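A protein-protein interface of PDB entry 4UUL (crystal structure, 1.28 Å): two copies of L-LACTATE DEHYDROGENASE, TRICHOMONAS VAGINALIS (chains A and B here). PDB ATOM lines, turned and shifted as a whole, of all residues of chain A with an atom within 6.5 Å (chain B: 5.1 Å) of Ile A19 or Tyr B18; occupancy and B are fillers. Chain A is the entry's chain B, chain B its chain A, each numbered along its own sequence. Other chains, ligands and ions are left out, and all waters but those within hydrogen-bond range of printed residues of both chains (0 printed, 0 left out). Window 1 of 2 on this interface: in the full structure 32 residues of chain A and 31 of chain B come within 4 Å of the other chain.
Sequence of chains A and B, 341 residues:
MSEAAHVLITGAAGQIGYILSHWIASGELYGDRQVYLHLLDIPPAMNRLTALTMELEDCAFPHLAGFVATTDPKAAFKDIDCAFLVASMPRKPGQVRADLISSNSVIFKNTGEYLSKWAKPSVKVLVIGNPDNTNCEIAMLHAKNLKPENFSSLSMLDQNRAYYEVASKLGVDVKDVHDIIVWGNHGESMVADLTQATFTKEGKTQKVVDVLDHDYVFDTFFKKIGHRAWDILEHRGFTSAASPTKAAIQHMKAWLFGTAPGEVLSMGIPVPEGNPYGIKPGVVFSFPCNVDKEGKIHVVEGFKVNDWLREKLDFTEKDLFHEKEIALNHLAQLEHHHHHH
OE1 of Glu B55 sits at hydrogen-bond distance from N of Ala A242 (3.2 Å). OE1 of Glu B55 lies within hydrogen-bond range of N of Ser A243, at 3.0 Å. The side-chain hydroxyl (OH) of Tyr B18 lies within hydrogen-bond range of the backbone NH (N) of Ala A241, 3.4 Å away. OE1 of Glu B55 lies within hydrogen-bond range of N of Ala A241. The side-chain carboxylate of Glu B55 lies within salt-bridge range of the guanidinium group of Arg A236 (3.8 Å). The backbone NH (N) of Ala A242 sits at hydrogen-bond distance from the side-chain hydroxyl (OH) of Tyr B18, at 2.9 Å.
O of Tyr A18 is in hydrogen-bond range of ND1 of His A22 (2.9 Å). The backbone carbonyl oxygen of Ala A241 lies within hydrogen-bond range of the side-chain hydroxyl of Thr A245. A ring nitrogen (ND1) of His B22 sits at hydrogen-bond distance from the backbone carbonyl oxygen (O) of Tyr B18. The side-chain carboxylate (OE2) of Glu B55 lies within hydrogen-bond range of the side-chain hydroxyl (OH) of Tyr B18 (2.6 Å). O of Tyr A18 lies within hydrogen-bond range of OG of Ser A21, 3.0 Å away. NE of Arg A236 lies within hydrogen-bond range of O of Thr A239, 2.9 Å away.
Among the printed residues, merely in contact across the chains: Tyr A18 with Ile B19, Ile A19 with Tyr B18, Arg A236 with Tyr B18, Ser A240 with Glu B55, Ala A242 with His B22 and Pro A244 with Glu B55.
Of chain B, only Tyr B18 comes within 4 Å of Ile A19. Tyr B18 touches four residues of chain A. Printed residues of chain A within 4 Å of Glu B55: Arg A236, Ser A240, Ala A241, Ala A242, Ser A243 and Pro A244. Of the printed residues of chain B, Ser A240 touches Glu B55 (3.3 Å). Of the printed residues of chain B, Pro A244 touches Glu B55. Of the printed residues of chain B, Ser A243 touches Glu B55 (3.0 Å). The nearest printed residue of chain B that does not touch Ile A19 is Ile B19 (4.6 Å). The nearest printed residue of chain A that does not touch Tyr B18 is Ser A240 (4.5 Å). The nearest printed residue of chain A that does not touch Glu B55 is Thr A239 (4.9 Å).
Hydrophobic or aromatic side chains of chain B within 4 Å of the printed part of chain A: Tyr B18, Ile B19 and His B22. Of the 22 printed residues of chain A, 8 touch a printed residue of chain B. Printed residues of chain A that touch a printed residue of chain B: Tyr A18, Ile A19, Arg A236, Ser A240, Ala A241, Ala A242, Ser A243 and Pro A244.
Tyr A18 touches Ile B19, and with the chains exchanged Ile A19 touches Tyr B18. Of the 12 pairs that touch across the chains among the printed residues, 2 have their exchanged pair printed and touching as well.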
ATOM      1  N   GLY A  14      23.389  10.757 -24.377  1.00  0.00           N
ATOM      2  CA  GLY A  14      22.348   9.773 -24.232  1.00  0.00           C
ATOM      3  C   GLY A  14      22.722   8.435 -24.795  1.00  0.00           C
ATOM      4  O   GLY A  14      23.827   8.239 -25.333  1.00  0.00           O
ATOM      5  N   GLN A  15      21.789   7.491 -24.736  1.00  0.00           N
ATOM      6  CA  GLN A  15      22.114   6.137 -25.193  1.00  0.00           C
ATOM      7  C   GLN A  15      22.384   6.055 -26.699  1.00  0.00           C
ATOM      8  O   GLN A  15      23.267   5.328 -27.125  1.00  0.00           O
ATOM      9  CB  GLN A  15      21.049   5.145 -24.798  1.00  0.00           C
ATOM     10  CG  GLN A  15      21.522   3.731 -25.055  1.00  0.00           C
ATOM     11  CD  GLN A  15      22.892   3.428 -24.450  1.00  0.00           C
ATOM     12  OE1 GLN A  15      23.809   3.047 -25.155  1.00  0.00           O
ATOM     13  NE2 GLN A  15      23.030   3.619 -23.140  1.00  0.00           N
ATOM     14  N   ILE A  16      21.572   6.758 -27.511  1.00  0.00           N
ATOM     15  CA  ILE A  16      21.832   6.752 -28.930  1.00  0.00           C
ATOM     16  C   ILE A  16      23.227   7.336 -29.185  1.00  0.00           C
ATOM     17  O   ILE A  16      24.052   6.758 -29.924  1.00  0.00           O
ATOM     18  CB  ILE A  16      20.739   7.475 -29.703  1.00  0.00           C
ATOM     19  CG1 ILE A  16      19.439   6.639 -29.654  1.00  0.00           C
ATOM     20  CG2 ILE A  16      21.194   7.733 -31.105  1.00  0.00           C
ATOM     21  CD1 ILE A  16      18.192   7.374 -30.167  1.00  0.00           C
ATOM     22  N   GLY A  17      23.531   8.463 -28.564  1.00  0.00           N
ATOM     23  CA  GLY A  17      24.817   9.071 -28.794  1.00  0.00           C
ATOM     24  C   GLY A  17      25.994   8.185 -28.442  1.00  0.00           C
ATOM     25  O   GLY A  17      27.038   8.182 -29.110  1.00  0.00           O
ATOM     26  N   TYR A  18      25.820   7.474 -27.345  1.00  0.00           N
ATOM     27  CA  TYR A  18      26.848   6.563 -26.837  1.00  0.00           C
ATOM     28  C   TYR A  18      27.172   5.529 -27.927  1.00  0.00           C
ATOM     29  O   TYR A  18      28.355   5.260 -28.243  1.00  0.00           O
ATOM     30  CB  TYR A  18      26.328   5.883 -25.594  1.00  0.00           C
ATOM     31  CG  TYR A  18      27.268   4.917 -24.907  1.00  0.00           C
ATOM     32  CD1 TYR A  18      28.361   5.361 -24.185  1.00  0.00           C
ATOM     33  CD2 TYR A  18      27.030   3.589 -24.923  1.00  0.00           C
ATOM     34  CE1 TYR A  18      29.211   4.483 -23.512  1.00  0.00           C
ATOM     35  CE2 TYR A  18      27.832   2.713 -24.248  1.00  0.00           C
ATOM     36  CZ  TYR A  18      28.915   3.158 -23.551  1.00  0.00           C
ATOM     37  OH  TYR A  18      29.643   2.246 -22.863  1.00  0.00           O
ATOM     38  N   ILE A  19      26.142   4.872 -28.454  1.00  0.00           N
ATOM     39  CA  ILE A  19      26.352   3.812 -29.419  1.00  0.00           C
ATOM     40  C   ILE A  19      26.824   4.399 -30.771  1.00  0.00           C
ATOM     41  O   ILE A  19      27.694   3.849 -31.440  1.00  0.00           O
ATOM     42  CB  ILE A  19      25.098   2.897 -29.586  1.00  0.00           C
ATOM     43  CG1 ILE A  19      24.701   2.288 -28.251  1.00  0.00           C
ATOM     44  CG2 ILE A  19      25.326   1.858 -30.646  1.00  0.00           C
ATOM     45  CD1 ILE A  19      23.379   1.605 -28.232  1.00  0.00           C
ATOM     46  N   LEU A  20      26.113   5.431 -31.212  1.00  0.00           N
ATOM     47  CA  LEU A  20      26.429   6.048 -32.481  1.00  0.00           C
ATOM     48  C   LEU A  20      27.868   6.535 -32.580  1.00  0.00           C
ATOM     49  O   LEU A  20      28.532   6.349 -33.597  1.00  0.00           O
ATOM     50  CB  LEU A  20      25.436   7.183 -32.692  1.00  0.00           C
ATOM     51  CG  LEU A  20      25.418   7.958 -33.962  1.00  0.00           C
ATOM     52  CD1 LEU A  20      25.153   7.049 -35.178  1.00  0.00           C
ATOM     53  CD2 LEU A  20      24.348   9.087 -33.853  1.00  0.00           C
ATOM     54  N   SER A  21      28.321   7.203 -31.545  1.00  0.00           N
ATOM     55  CA  SER A  21      29.690   7.687 -31.548  1.00  0.00           C
ATOM     56  C   SER A  21      30.691   6.559 -31.684  1.00  0.00           C
ATOM     57  O   SER A  21      31.606   6.667 -32.482  1.00  0.00           O
ATOM     58  CB  SER A  21      29.987   8.528 -30.306  1.00  0.00           C
ATOM     59  OG  SER A  21      29.830   7.774 -29.113  1.00  0.00           O
ATOM     60  N   HIS A  22      30.502   5.482 -30.933  1.00  0.00           N
ATOM     61  CA  HIS A  22      31.435   4.371 -31.060  1.00  0.00           C
ATOM     62  C   HIS A  22      31.366   3.689 -32.433  1.00  0.00           C
ATOM     63  O   HIS A  22      32.384   3.331 -33.017  1.00  0.00           O
ATOM     64  CB  HIS A  22      31.194   3.346 -29.950  1.00  0.00           C
ATOM     65  CG  HIS A  22      31.761   3.718 -28.614  1.00  0.00           C
ATOM     66  ND1 HIS A  22      31.104   4.514 -27.711  1.00  0.00           N
ATOM     67  CD2 HIS A  22      32.942   3.388 -28.028  1.00  0.00           C
ATOM     68  CE1 HIS A  22      31.874   4.682 -26.644  1.00  0.00           C
ATOM     69  NE2 HIS A  22      32.988   4.016 -26.820  1.00  0.00           N
ATOM     70  N   TRP A  23      30.164   3.574 -32.955  1.00  0.00           N
ATOM     71  CA  TRP A  23      29.960   2.901 -34.220  1.00  0.00           C
ATOM     72  C   TRP A  23      30.638   3.696 -35.318  1.00  0.00           C
ATOM     73  O   TRP A  23      31.372   3.156 -36.137  1.00  0.00           O
ATOM     74  CB  TRP A  23      28.471   2.726 -34.462  1.00  0.00           C
ATOM     75  CG  TRP A  23      28.077   1.525 -35.325  1.00  0.00           C
ATOM     76  CD1 TRP A  23      28.878   0.833 -36.177  1.00  0.00           C
ATOM     77  CD2 TRP A  23      26.806   0.848 -35.346  1.00  0.00           C
ATOM     78  NE1 TRP A  23      28.168  -0.178 -36.798  1.00  0.00           N
ATOM     79  CE2 TRP A  23      26.900  -0.205 -36.283  1.00  0.00           C
ATOM     80  CE3 TRP A  23      25.611   1.034 -34.671  1.00  0.00           C
ATOM     81  CZ2 TRP A  23      25.846  -1.069 -36.544  1.00  0.00           C
ATOM     82  CZ3 TRP A  23      24.563   0.177 -34.940  1.00  0.00           C
ATOM     83  CH2 TRP A  23      24.685  -0.849 -35.869  1.00  0.00           C
ATOM     84  N   ILE A  24      30.439   5.000 -35.312  1.00  0.00           N
ATOM     85  CA  ILE A  24      31.088   5.868 -36.297  1.00  0.00           C
ATOM     86  C   ILE A  24      32.620   5.837 -36.133  1.00  0.00           C
ATOM     87  O   ILE A  24      33.375   5.739 -37.114  1.00  0.00           O
ATOM     88  CB  ILE A  24      30.556   7.302 -36.198  1.00  0.00           C
ATOM     89  CG1 ILE A  24      29.086   7.315 -36.670  1.00  0.00           C
ATOM     90  CG2 ILE A  24      31.375   8.252 -37.087  1.00  0.00           C
ATOM     91  CD1 ILE A  24      28.361   8.561 -36.387  1.00  0.00           C
ATOM     92  N   LEU A  52      31.650   9.118 -21.862  1.00  0.00           N
ATOM     93  CA  LEU A  52      31.617   8.644 -23.257  1.00  0.00           C
ATOM     94  C   LEU A  52      32.984   8.835 -23.902  1.00  0.00           C
ATOM     95  O   LEU A  52      33.513   7.940 -24.523  1.00  0.00           O
ATOM     96  CB  LEU A  52      30.500   9.320 -24.087  1.00  0.00           C
ATOM     97  CG  LEU A  52      30.745   9.298 -25.614  1.00  0.00           C
ATOM     98  CD1 LEU A  52      30.706   7.905 -26.083  1.00  0.00           C
ATOM     99  CD2 LEU A  52      29.651  10.105 -26.313  1.00  0.00           C
ATOM    100  N   ARG A 236      11.922  -3.135 -21.808  1.00  0.00           N
ATOM    101  CA  ARG A 236      13.298  -2.614 -21.602  1.00  0.00           C
ATOM    102  C   ARG A 236      13.409  -1.646 -20.436  1.00  0.00           C
ATOM    103  O   ARG A 236      14.453  -1.599 -19.770  1.00  0.00           O
ATOM    104  CB  ARG A 236      13.784  -1.917 -22.885  1.00  0.00           C
ATOM    105  CG  ARG A 236      15.201  -1.295 -22.904  1.00  0.00           C
ATOM    106  CD  ARG A 236      15.514  -0.833 -24.336  1.00  0.00           C
ATOM    107  NE  ARG A 236      16.434   0.305 -24.424  1.00  0.00           N
ATOM    108  CZ  ARG A 236      17.739   0.230 -24.181  1.00  0.00           C
ATOM    109  NH1 ARG A 236      18.290  -0.921 -23.838  1.00  0.00           N
ATOM    110  NH2 ARG A 236      18.490   1.308 -24.279  1.00  0.00           N
ATOM    111  N   THR A 239      13.470   3.571 -23.872  1.00  0.00           N
ATOM    112  CA  THR A 239      13.174   3.488 -25.315  1.00  0.00           C
ATOM    113  C   THR A 239      14.317   2.874 -26.082  1.00  0.00           C
ATOM    114  O   THR A 239      15.397   2.731 -25.560  1.00  0.00           O
ATOM    115  CB  THR A 239      12.870   4.871 -25.899  1.00  0.00           C
ATOM    116  OG1 THR A 239      13.985   5.737 -25.690  1.00  0.00           O
ATOM    117  CG2 THR A 239      11.675   5.471 -25.213  1.00  0.00           C
ATOM    118  N   SER A 240      14.055   2.545 -27.340  1.00  0.00           N
ATOM    119  CA  SER A 240      15.040   1.917 -28.196  1.00  0.00           C
ATOM    120  C   SER A 240      16.250   2.834 -28.392  1.00  0.00           C
ATOM    121  O   SER A 240      16.158   4.064 -28.314  1.00  0.00           O
ATOM    122  CB  SER A 240      14.408   1.525 -29.533  1.00  0.00           C
ATOM    123  OG  SER A 240      13.422   0.499 -29.377  1.00  0.00           O
ATOM    124  N   ALA A 241      17.389   2.207 -28.619  1.00  0.00           N
ATOM    125  CA  ALA A 241      18.643   2.931 -28.818  1.00  0.00           C
ATOM    126  C   ALA A 241      19.489   2.306 -29.934  1.00  0.00           C
ATOM    127  O   ALA A 241      19.862   2.967 -30.898  1.00  0.00           O
ATOM    128  CB  ALA A 241      19.401   3.056 -27.529  1.00  0.00           C
ATOM    129  N   ALA A 242      19.811   1.015 -29.820  1.00  0.00           N
ATOM    130  CA  ALA A 242      20.579   0.361 -30.847  1.00  0.00           C
ATOM    131  C   ALA A 242      19.876   0.346 -32.186  1.00  0.00           C
ATOM    132  O   ALA A 242      20.528   0.555 -33.203  1.00  0.00           O
ATOM    133  CB  ALA A 242      20.945  -1.042 -30.439  1.00  0.00           C
ATOM    134  N   SER A 243      18.565   0.113 -32.219  1.00  0.00           N
ATOM    135  CA  SER A 243      17.853   0.038 -33.492  1.00  0.00           C
ATOM    136  C   SER A 243      17.735   1.391 -34.221  1.00  0.00           C
ATOM    137  O   SER A 243      17.969   1.428 -35.424  1.00  0.00           O
ATOM    138  CB  SER A 243      16.533  -0.746 -33.397  1.00  0.00           C
ATOM    139  OG  SER A 243      15.683  -0.143 -32.469  1.00  0.00           O
ATOM    140  N   PRO A 244      17.396   2.497 -33.522  1.00  0.00           N
ATOM    141  CA  PRO A 244      17.451   3.786 -34.258  1.00  0.00           C
ATOM    142  C   PRO A 244      18.864   4.140 -34.668  1.00  0.00           C
ATOM    143  O   PRO A 244      19.044   4.751 -35.715  1.00  0.00           O
ATOM    144  CB  PRO A 244      16.846   4.794 -33.283  1.00  0.00           C
ATOM    145  CG  PRO A 244      16.894   4.145 -31.942  1.00  0.00           C
ATOM    146  CD  PRO A 244      16.774   2.662 -32.198  1.00  0.00           C
ATOM    147  N   THR A 245      19.867   3.743 -33.884  1.00  0.00           N
ATOM    148  CA  THR A 245      21.241   4.044 -34.254  1.00  0.00           C
ATOM    149  C   THR A 245      21.608   3.317 -35.545  1.00  0.00           C
ATOM    150  O   THR A 245      22.215   3.887 -36.455  1.00  0.00           O
ATOM    151  CB  THR A 245      22.210   3.657 -33.132  1.00  0.00           C
ATOM    152  OG1 THR A 245      21.969   4.451 -31.960  1.00  0.00           O
ATOM    153  CG2 THR A 245      23.636   3.883 -33.554  1.00  0.00           C
ATOM    154  N   LYS A 246      21.241   2.034 -35.636  1.00  0.00           N
ATOM    155  CA  LYS A 246      21.500   1.215 -36.814  1.00  0.00           C
ATOM    156  C   LYS A 246      20.871   1.905 -38.039  1.00  0.00           C
ATOM    157  O   LYS A 246      21.482   2.040 -39.088  1.00  0.00           O
ATOM    158  CB  LYS A 246      20.986  -0.191 -36.593  1.00  0.00           C
ATOM    159  CG  LYS A 246      21.291  -1.187 -37.721  1.00  0.00           C
ATOM    160  CD  LYS A 246      20.335  -1.188 -38.876  1.00  0.00           C
ATOM    161  CE  LYS A 246      20.788  -2.195 -39.936  1.00  0.00           C
ATOM    162  NZ  LYS A 246      19.812  -2.312 -41.040  1.00  0.00           N
ATOM    163  N   ILE A 249      22.771   5.356 -38.982  1.00  0.00           N
ATOM    164  CA  ILE A 249      24.006   5.101 -39.718  1.00  0.00           C
ATOM    165  C   ILE A 249      23.705   4.638 -41.122  1.00  0.00           C
ATOM    166  O   ILE A 249      24.302   5.131 -42.079  1.00  0.00           O
ATOM    167  CB  ILE A 249      24.908   4.109 -38.976  1.00  0.00           C
ATOM    168  CG1 ILE A 249      25.419   4.792 -37.692  1.00  0.00           C
ATOM    169  CG2 ILE A 249      26.087   3.614 -39.851  1.00  0.00           C
ATOM    170  CD1 ILE A 249      26.115   3.862 -36.776  1.00  0.00           C
ATOM    171  N   ALA B  12      23.420 -11.809 -21.568  1.00  0.00           N
ATOM    172  CA  ALA B  12      23.058 -11.136 -22.802  1.00  0.00           C
ATOM    173  C   ALA B  12      22.178  -9.919 -22.605  1.00  0.00           C
ATOM    174  O   ALA B  12      22.164  -9.052 -23.475  1.00  0.00           O
ATOM    175  CB  ALA B  12      22.440 -12.106 -23.812  1.00  0.00           C
ATOM    176  N   GLY B  14      22.498  -7.636 -20.352  1.00  0.00           N
ATOM    177  CA  GLY B  14      23.225  -6.529 -19.803  1.00  0.00           C
ATOM    178  C   GLY B  14      23.699  -5.551 -20.870  1.00  0.00           C
ATOM    179  O   GLY B  14      23.454  -5.713 -22.065  1.00  0.00           O
ATOM    180  N   GLN B  15      24.422  -4.521 -20.439  1.00  0.00           N
ATOM    181  CA  GLN B  15      24.843  -3.476 -21.334  1.00  0.00           C
ATOM    182  C   GLN B  15      25.841  -3.968 -22.379  1.00  0.00           C
ATOM    183  O   GLN B  15      25.762  -3.582 -23.550  1.00  0.00           O
ATOM    184  CB  GLN B  15      25.496  -2.326 -20.544  1.00  0.00           C
ATOM    185  CG  GLN B  15      24.700  -1.729 -19.415  1.00  0.00           C
ATOM    186  CD  GLN B  15      25.426  -0.518 -18.778  1.00  0.00           C
ATOM    187  OE1 GLN B  15      26.657  -0.541 -18.536  1.00  0.00           O
ATOM    188  NE2 GLN B  15      24.665   0.545 -18.513  1.00  0.00           N
ATOM    189  N   ILE B  16      26.818  -4.769 -21.963  1.00  0.00           N
ATOM    190  CA  ILE B  16      27.745  -5.328 -22.933  1.00  0.00           C
ATOM    191  C   ILE B  16      26.985  -6.198 -23.924  1.00  0.00           C
ATOM    192  O   ILE B  16      27.169  -6.067 -25.123  1.00  0.00           O
ATOM    193  CB  ILE B  16      28.879  -6.108 -22.253  1.00  0.00           C
ATOM    194  CG1 ILE B  16      29.850  -5.120 -21.539  1.00  0.00           C
ATOM    195  CG2 ILE B  16      29.636  -6.935 -23.250  1.00  0.00           C
ATOM    196  CD1 ILE B  16      30.858  -5.761 -20.595  1.00  0.00           C
ATOM    197  N   GLY B  17      26.149  -7.094 -23.426  1.00  0.00           N
ATOM    198  CA  GLY B  17      25.380  -7.957 -24.297  1.00  0.00           C
ATOM    199  C   GLY B  17      24.540  -7.211 -25.333  1.00  0.00           C
ATOM    200  O   GLY B  17      24.437  -7.642 -26.488  1.00  0.00           O
ATOM    201  N   TYR B  18      23.953  -6.116 -24.897  1.00  0.00           N
ATOM    202  CA  TYR B  18      23.114  -5.294 -25.764  1.00  0.00           C
ATOM    203  C   TYR B  18      23.929  -4.814 -26.966  1.00  0.00           C
ATOM    204  O   TYR B  18      23.489  -4.918 -28.127  1.00  0.00           O
ATOM    205  CB  TYR B  18      22.613  -4.127 -24.941  1.00  0.00           C
ATOM    206  CG  TYR B  18      21.669  -3.180 -25.648  1.00  0.00           C
ATOM    207  CD1 TYR B  18      20.350  -3.509 -25.898  1.00  0.00           C
ATOM    208  CD2 TYR B  18      22.085  -1.923 -26.041  1.00  0.00           C
ATOM    209  CE1 TYR B  18      19.480  -2.609 -26.491  1.00  0.00           C
ATOM    210  CE2 TYR B  18      21.223  -1.031 -26.632  1.00  0.00           C
ATOM    211  CZ  TYR B  18      19.935  -1.378 -26.873  1.00  0.00           C
ATOM    212  OH  TYR B  18      19.098  -0.455 -27.436  1.00  0.00           O
ATOM    213  N   ILE B  19      25.091  -4.211 -26.703  1.00  0.00           N
ATOM    214  CA  ILE B  19      25.886  -3.659 -27.787  1.00  0.00           C
ATOM    215  C   ILE B  19      26.566  -4.789 -28.610  1.00  0.00           C
ATOM    216  O   ILE B  19      26.620  -4.728 -29.842  1.00  0.00           O
ATOM    217  CB  ILE B  19      26.945  -2.670 -27.243  1.00  0.00           C
ATOM    218  CG1 ILE B  19      26.263  -1.579 -26.423  1.00  0.00           C
ATOM    219  CG2 ILE B  19      27.804  -2.135 -28.347  1.00  0.00           C
ATOM    220  CD1 ILE B  19      27.208  -0.699 -25.734  1.00  0.00           C
ATOM    221  N   LEU B  20      27.144  -5.765 -27.900  1.00  0.00           N
ATOM    222  CA  LEU B  20      27.829  -6.878 -28.559  1.00  0.00           C
ATOM    223  C   LEU B  20      26.928  -7.624 -29.538  1.00  0.00           C
ATOM    224  O   LEU B  20      27.330  -7.940 -30.651  1.00  0.00           O
ATOM    225  CB  LEU B  20      28.369  -7.801 -27.484  1.00  0.00           C
ATOM    226  CG  LEU B  20      29.231  -8.969 -27.896  1.00  0.00           C
ATOM    227  CD1 LEU B  20      30.488  -8.569 -28.673  1.00  0.00           C
ATOM    228  CD2 LEU B  20      29.613  -9.755 -26.643  1.00  0.00           C
ATOM    229  N   SER B  21      25.701  -7.892 -29.111  1.00  0.00           N
ATOM    230  CA  SER B  21      24.736  -8.593 -29.949  1.00  0.00           C
ATOM    231  C   SER B  21      24.502  -7.871 -31.267  1.00  0.00           C
ATOM    232  O   SER B  21      24.520  -8.444 -32.344  1.00  0.00           O
ATOM    233  CB  SER B  21      23.396  -8.728 -29.209  1.00  0.00           C
ATOM    234  OG  SER B  21      23.438  -9.714 -28.204  1.00  0.00           O
ATOM    235  N   HIS B  22      24.244  -6.579 -31.156  1.00  0.00           N
ATOM    236  CA  HIS B  22      23.962  -5.784 -32.338  1.00  0.00           C
ATOM    237  C   HIS B  22      25.204  -5.651 -33.251  1.00  0.00           C
ATOM    238  O   HIS B  22      25.105  -5.764 -34.467  1.00  0.00           O
ATOM    239  CB  HIS B  22      23.487  -4.376 -31.920  1.00  0.00           C
ATOM    240  CG  HIS B  22      22.043  -4.331 -31.551  1.00  0.00           C
ATOM    241  ND1 HIS B  22      21.592  -4.588 -30.274  1.00  0.00           N
ATOM    242  CD2 HIS B  22      20.945  -4.003 -32.276  1.00  0.00           C
ATOM    243  CE1 HIS B  22      20.263  -4.482 -30.250  1.00  0.00           C
ATOM    244  NE2 HIS B  22      19.852  -4.134 -31.453  1.00  0.00           N
ATOM    245  N   LEU B  52      15.756  -6.928 -25.882  1.00  0.00           N
ATOM    246  CA  LEU B  52      16.914  -6.971 -26.784  1.00  0.00           C
ATOM    247  C   LEU B  52      16.567  -7.648 -28.098  1.00  0.00           C
ATOM    248  O   LEU B  52      16.899  -7.148 -29.185  1.00  0.00           O
ATOM    249  CB  LEU B  52      18.087  -7.671 -26.083  1.00  0.00           C
ATOM    250  CG  LEU B  52      19.251  -8.067 -27.019  1.00  0.00           C
ATOM    251  CD1 LEU B  52      19.863  -6.875 -27.674  1.00  0.00           C
ATOM    252  CD2 LEU B  52      20.319  -8.817 -26.254  1.00  0.00           C
ATOM    253  N   GLU B  55      14.684  -5.316 -30.459  1.00  0.00           N
ATOM    254  CA  GLU B  55      15.522  -4.384 -31.193  1.00  0.00           C
ATOM    255  C   GLU B  55      16.364  -5.057 -32.245  1.00  0.00           C
ATOM    256  O   GLU B  55      16.552  -4.458 -33.324  1.00  0.00           O
ATOM    257  CB  GLU B  55      16.376  -3.481 -30.293  1.00  0.00           C
ATOM    258  CG  GLU B  55      15.586  -2.405 -29.580  1.00  0.00           C
ATOM    259  CD  GLU B  55      16.461  -1.343 -29.038  1.00  0.00           C
ATOM    260  OE1 GLU B  55      16.956  -0.485 -29.814  1.00  0.00           O
ATOM    261  OE2 GLU B  55      16.716  -1.379 -27.823  1.00  0.00           O
